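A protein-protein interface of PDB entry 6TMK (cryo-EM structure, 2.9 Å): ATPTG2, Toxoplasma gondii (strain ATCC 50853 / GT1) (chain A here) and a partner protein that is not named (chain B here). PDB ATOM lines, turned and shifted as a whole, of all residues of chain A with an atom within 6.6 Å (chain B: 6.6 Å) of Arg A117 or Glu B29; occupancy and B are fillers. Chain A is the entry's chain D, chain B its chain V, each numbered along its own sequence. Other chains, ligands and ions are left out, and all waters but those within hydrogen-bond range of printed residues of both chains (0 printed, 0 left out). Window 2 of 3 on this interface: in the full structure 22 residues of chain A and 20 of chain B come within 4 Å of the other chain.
The backbone NH (N) of Lys B31 is in hydrogen-bond range of the side-chain carboxylate (OD1) of Asp A115. OD2 of Asp A115 lies close to O of Met B28 (3.0 Å). The backbone NH (N) of Gly B30 lies within hydrogen-bond range of the side-chain carboxylate (OD1) of Asp A115. NH1 of Arg A117 is in hydrogen-bond range of O of Trp B25. The side-chain carboxylate of Glu B29 is in salt-bridge range of the guanidinium group of Arg A117 (3.5 Å). The backbone NH (N) of Leu A116 sits close to the backbone carbonyl oxygen (O) of Lys B31.
OD2 of Asp A115 lies close to N of Arg A117 (3.5 Å).
Among the printed residues, merely in contact across the chains: Asp A115 with Glu B29, Leu A116 with Met B28, Arg A117 with Arg B26 and Val A121 with Trp B25.
Arg A117 touches just these residues of chain B: Trp B25, Arg B26 and Glu B29. Of chain A, only Asp A115 (3.8 Å) and Arg A117 (3.5 Å) come within 4 Å of Glu B29. Printed residues of chain A within 4 Å of Gly B30: Asp A115 (3.0 Å). Printed residues of chain A within 4 Å of Met B28: Asp A115 and Leu A116. Ala B24 touches none of the printed residues of chain A. Leu A118 touches none of the printed residues of chain B.
Printed residues of chain A that touch a printed residue of chain B: Asp A115, Leu A116, Arg A117 and Val A121. Hydrophobic or aromatic side chains of chain A within 4 Å of the printed part of chain B: Leu A116 and Val A121. Of the 8 printed residues of chain B, 6 touch a printed residue of chain A. Among the printed residues, 10 pairs touch across the chains. Among the printed residues, Asp or Glu carboxylates within 4 Å of a Lys or Arg side-chain nitrogen of the other chain: Arg A117 with Glu B29 (3.5 Å).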
ATOM      1  N   ASP A 115      17.009   8.845  31.960  1.00  0.00           N
ATOM      2  CA  ASP A 115      17.002   8.569  30.533  1.00  0.00           C
ATOM      3  C   ASP A 115      17.656   7.228  30.227  1.00  0.00           C
ATOM      4  O   ASP A 115      18.407   6.670  31.030  1.00  0.00           O
ATOM      5  CB  ASP A 115      17.720   9.684  29.765  1.00  0.00           C
ATOM      6  CG  ASP A 115      17.271   9.777  28.323  1.00  0.00           C
ATOM      7  OD1 ASP A 115      16.174  10.320  28.076  1.00  0.00           O
ATOM      8  OD2 ASP A 115      18.011   9.306  27.436  1.00  0.00           O
ATOM      9  N   LEU A 116      17.352   6.721  29.030  1.00  0.00           N
ATOM     10  CA  LEU A 116      17.836   5.406  28.632  1.00  0.00           C
ATOM     11  C   LEU A 116      19.353   5.385  28.513  1.00  0.00           C
ATOM     12  O   LEU A 116      19.997   4.403  28.897  1.00  0.00           O
ATOM     13  CB  LEU A 116      17.200   4.997  27.307  1.00  0.00           C
ATOM     14  CG  LEU A 116      17.836   3.806  26.587  1.00  0.00           C
ATOM     15  CD1 LEU A 116      17.718   2.548  27.416  1.00  0.00           C
ATOM     16  CD2 LEU A 116      17.218   3.608  25.226  1.00  0.00           C
ATOM     17  N   ARG A 117      19.941   6.443  27.956  1.00  0.00           N
ATOM     18  CA  ARG A 117      21.389   6.456  27.787  1.00  0.00           C
ATOM     19  C   ARG A 117      22.088   6.449  29.139  1.00  0.00           C
ATOM     20  O   ARG A 117      23.107   5.772  29.322  1.00  0.00           O
ATOM     21  CB  ARG A 117      21.811   7.670  26.961  1.00  0.00           C
ATOM     22  CG  ARG A 117      21.377   8.996  27.539  1.00  0.00           C
ATOM     23  CD  ARG A 117      22.156  10.145  26.933  1.00  0.00           C
ATOM     24  NE  ARG A 117      21.770  10.413  25.555  1.00  0.00           N
ATOM     25  CZ  ARG A 117      22.236  11.432  24.842  1.00  0.00           C
ATOM     26  NH1 ARG A 117      21.835  11.608  23.597  1.00  0.00           N
ATOM     27  NH2 ARG A 117      23.108  12.273  25.375  1.00  0.00           N
ATOM     28  N   LEU A 118      21.523   7.159  30.115  1.00  0.00           N
ATOM     29  CA  LEU A 118      22.103   7.172  31.449  1.00  0.00           C
ATOM     30  C   LEU A 118      21.915   5.827  32.136  1.00  0.00           C
ATOM     31  O   LEU A 118      22.803   5.362  32.859  1.00  0.00           O
ATOM     32  CB  LEU A 118      21.475   8.288  32.276  1.00  0.00           C
ATOM     33  CG  LEU A 118      21.451   9.667  31.620  1.00  0.00           C
ATOM     34  CD1 LEU A 118      20.825  10.679  32.550  1.00  0.00           C
ATOM     35  CD2 LEU A 118      22.839  10.109  31.227  1.00  0.00           C
ATOM     36  N   GLN A 119      20.768   5.187  31.918  1.00  0.00           N
ATOM     37  CA  GLN A 119      20.559   3.850  32.458  1.00  0.00           C
ATOM     38  C   GLN A 119      21.574   2.870  31.889  1.00  0.00           C
ATOM     39  O   GLN A 119      22.132   2.043  32.621  1.00  0.00           O
ATOM     40  CB  GLN A 119      19.139   3.389  32.155  1.00  0.00           C
ATOM     41  CG  GLN A 119      18.099   4.001  33.059  1.00  0.00           C
ATOM     42  CD  GLN A 119      16.718   3.979  32.459  1.00  0.00           C
ATOM     43  OE1 GLN A 119      16.420   3.172  31.581  1.00  0.00           O
ATOM     44  NE2 GLN A 119      15.861   4.870  32.932  1.00  0.00           N
ATOM     45  N   PHE A 120      21.827   2.950  30.585  1.00  0.00           N
ATOM     46  CA  PHE A 120      22.800   2.066  29.958  1.00  0.00           C
ATOM     47  C   PHE A 120      24.199   2.337  30.492  1.00  0.00           C
ATOM     48  O   PHE A 120      24.970   1.402  30.748  1.00  0.00           O
ATOM     49  CB  PHE A 120      22.745   2.237  28.440  1.00  0.00           C
ATOM     50  CG  PHE A 120      23.827   1.508  27.704  1.00  0.00           C
ATOM     51  CD1 PHE A 120      23.893   0.126  27.725  1.00  0.00           C
ATOM     52  CD2 PHE A 120      24.773   2.205  26.977  1.00  0.00           C
ATOM     53  CE1 PHE A 120      24.889  -0.542  27.042  1.00  0.00           C
ATOM     54  CE2 PHE A 120      25.769   1.542  26.294  1.00  0.00           C
ATOM     55  CZ  PHE A 120      25.825   0.169  26.325  1.00  0.00           C
ATOM     56  N   VAL A 121      24.542   3.612  30.681  1.00  0.00           N
ATOM     57  CA  VAL A 121      25.846   3.955  31.234  1.00  0.00           C
ATOM     58  C   VAL A 121      25.998   3.384  32.636  1.00  0.00           C
ATOM     59  O   VAL A 121      27.043   2.821  32.986  1.00  0.00           O
ATOM     60  CB  VAL A 121      26.031   5.482  31.226  1.00  0.00           C
ATOM     61  CG1 VAL A 121      27.167   5.886  32.130  1.00  0.00           C
ATOM     62  CG2 VAL A 121      26.274   5.973  29.826  1.00  0.00           C
ATOM     63  N   ALA A 122      24.962   3.526  33.464  1.00  0.00           N
ATOM     64  CA  ALA A 122      25.034   3.024  34.830  1.00  0.00           C
ATOM     65  C   ALA A 122      25.151   1.508  34.849  1.00  0.00           C
ATOM     66  O   ALA A 122      25.915   0.945  35.641  1.00  0.00           O
ATOM     67  CB  ALA A 122      23.809   3.476  35.616  1.00  0.00           C
ATOM     68  N   ALA B  24      23.228   7.104  17.061  1.00  0.00           N
ATOM     69  CA  ALA B  24      22.303   6.452  17.981  1.00  0.00           C
ATOM     70  C   ALA B  24      22.368   7.074  19.366  1.00  0.00           C
ATOM     71  O   ALA B  24      21.349   7.183  20.052  1.00  0.00           O
ATOM     72  CB  ALA B  24      22.611   4.961  18.052  1.00  0.00           C
ATOM     73  N   TRP B  25      23.564   7.467  19.801  1.00  0.00           N
ATOM     74  CA  TRP B  25      23.695   8.186  21.061  1.00  0.00           C
ATOM     75  C   TRP B  25      22.850   9.450  21.058  1.00  0.00           C
ATOM     76  O   TRP B  25      22.164   9.752  22.040  1.00  0.00           O
ATOM     77  CB  TRP B  25      25.159   8.516  21.319  1.00  0.00           C
ATOM     78  CG  TRP B  25      25.400   9.162  22.632  1.00  0.00           C
ATOM     79  CD1 TRP B  25      25.654  10.479  22.864  1.00  0.00           C
ATOM     80  CD2 TRP B  25      25.413   8.520  23.908  1.00  0.00           C
ATOM     81  NE1 TRP B  25      25.823  10.699  24.207  1.00  0.00           N
ATOM     82  CE2 TRP B  25      25.680   9.509  24.870  1.00  0.00           C
ATOM     83  CE3 TRP B  25      25.224   7.204  24.330  1.00  0.00           C
ATOM     84  CZ2 TRP B  25      25.761   9.224  26.225  1.00  0.00           C
ATOM     85  CZ3 TRP B  25      25.307   6.924  25.675  1.00  0.00           C
ATOM     86  CH2 TRP B  25      25.572   7.927  26.608  1.00  0.00           C
ATOM     87  N   ARG B  26      22.888  10.201  19.959  1.00  0.00           N
ATOM     88  CA  ARG B  26      22.069  11.405  19.873  1.00  0.00           C
ATOM     89  C   ARG B  26      20.584  11.066  19.785  1.00  0.00           C
ATOM     90  O   ARG B  26      19.752  11.756  20.385  1.00  0.00           O
ATOM     91  CB  ARG B  26      22.503  12.245  18.676  1.00  0.00           C
ATOM     92  CG  ARG B  26      23.810  12.970  18.896  1.00  0.00           C
ATOM     93  CD  ARG B  26      24.156  13.893  17.742  1.00  0.00           C
ATOM     94  NE  ARG B  26      25.569  13.805  17.371  1.00  0.00           N
ATOM     95  CZ  ARG B  26      26.042  13.163  16.306  1.00  0.00           C
ATOM     96  NH1 ARG B  26      27.346  13.152  16.074  1.00  0.00           N
ATOM     97  NH2 ARG B  26      25.230  12.536  15.468  1.00  0.00           N
ATOM     98  N   ARG B  27      20.227  10.018  19.042  1.00  0.00           N
ATOM     99  CA  ARG B  27      18.825   9.631  18.934  1.00  0.00           C
ATOM    100  C   ARG B  27      18.253   9.108  20.246  1.00  0.00           C
ATOM    101  O   ARG B  27      17.034   9.164  20.440  1.00  0.00           O
ATOM    102  CB  ARG B  27      18.646   8.571  17.851  1.00  0.00           C
ATOM    103  CG  ARG B  27      18.362   9.134  16.477  1.00  0.00           C
ATOM    104  CD  ARG B  27      17.875   8.064  15.513  1.00  0.00           C
ATOM    105  NE  ARG B  27      18.972   7.325  14.889  1.00  0.00           N
ATOM    106  CZ  ARG B  27      19.336   6.084  15.206  1.00  0.00           C
ATOM    107  NH1 ARG B  27      20.347   5.519  14.566  1.00  0.00           N
ATOM    108  NH2 ARG B  27      18.706   5.404  16.153  1.00  0.00           N
ATOM    109  N   MET B  28      19.091   8.602  21.144  1.00  0.00           N
ATOM    110  CA  MET B  28      18.612   8.060  22.409  1.00  0.00           C
ATOM    111  C   MET B  28      18.232   9.133  23.417  1.00  0.00           C
ATOM    112  O   MET B  28      17.811   8.793  24.528  1.00  0.00           O
ATOM    113  CB  MET B  28      19.671   7.150  23.034  1.00  0.00           C
ATOM    114  CG  MET B  28      19.624   5.712  22.558  1.00  0.00           C
ATOM    115  SD  MET B  28      20.325   4.566  23.762  1.00  0.00           S
ATOM    116  CE  MET B  28      22.016   4.449  23.195  1.00  0.00           C
ATOM    117  N   GLU B  29      18.364  10.408  23.070  1.00  0.00           N
ATOM    118  CA  GLU B  29      18.005  11.469  23.997  1.00  0.00           C
ATOM    119  C   GLU B  29      16.489  11.532  24.132  1.00  0.00           C
ATOM    120  O   GLU B  29      15.769  11.621  23.134  1.00  0.00           O
ATOM    121  CB  GLU B  29      18.559  12.805  23.513  1.00  0.00           C
ATOM    122  CG  GLU B  29      18.397  13.945  24.505  1.00  0.00           C
ATOM    123  CD  GLU B  29      19.183  13.720  25.783  1.00  0.00           C
ATOM    124  OE1 GLU B  29      20.294  14.278  25.905  1.00  0.00           O
ATOM    125  OE2 GLU B  29      18.692  12.985  26.666  1.00  0.00           O
ATOM    126  N   GLY B  30      16.004  11.486  25.370  1.00  0.00           N
ATOM    127  CA  GLY B  30      14.575  11.488  25.603  1.00  0.00           C
ATOM    128  C   GLY B  30      13.917  10.264  25.005  1.00  0.00           C
ATOM    129  O   GLY B  30      13.117  10.365  24.070  1.00  0.00           O
ATOM    130  N   LYS B  31      14.258   9.098  25.543  1.00  0.00           N
ATOM    131  CA  LYS B  31      13.835   7.826  24.980  1.00  0.00           C
ATOM    132  C   LYS B  31      13.843   6.795  26.095  1.00  0.00           C
ATOM    133  O   LYS B  31      14.613   6.908  27.051  1.00  0.00           O
ATOM    134  CB  LYS B  31      14.755   7.396  23.835  1.00  0.00           C
ATOM    135  CG  LYS B  31      14.335   6.126  23.111  1.00  0.00           C
ATOM    136  CD  LYS B  31      12.981   6.255  22.432  1.00  0.00           C
ATOM    137  CE  LYS B  31      13.024   7.236  21.276  1.00  0.00           C
ATOM    138  NZ  LYS B  31      13.899   6.751  20.177  1.00  0.00           N
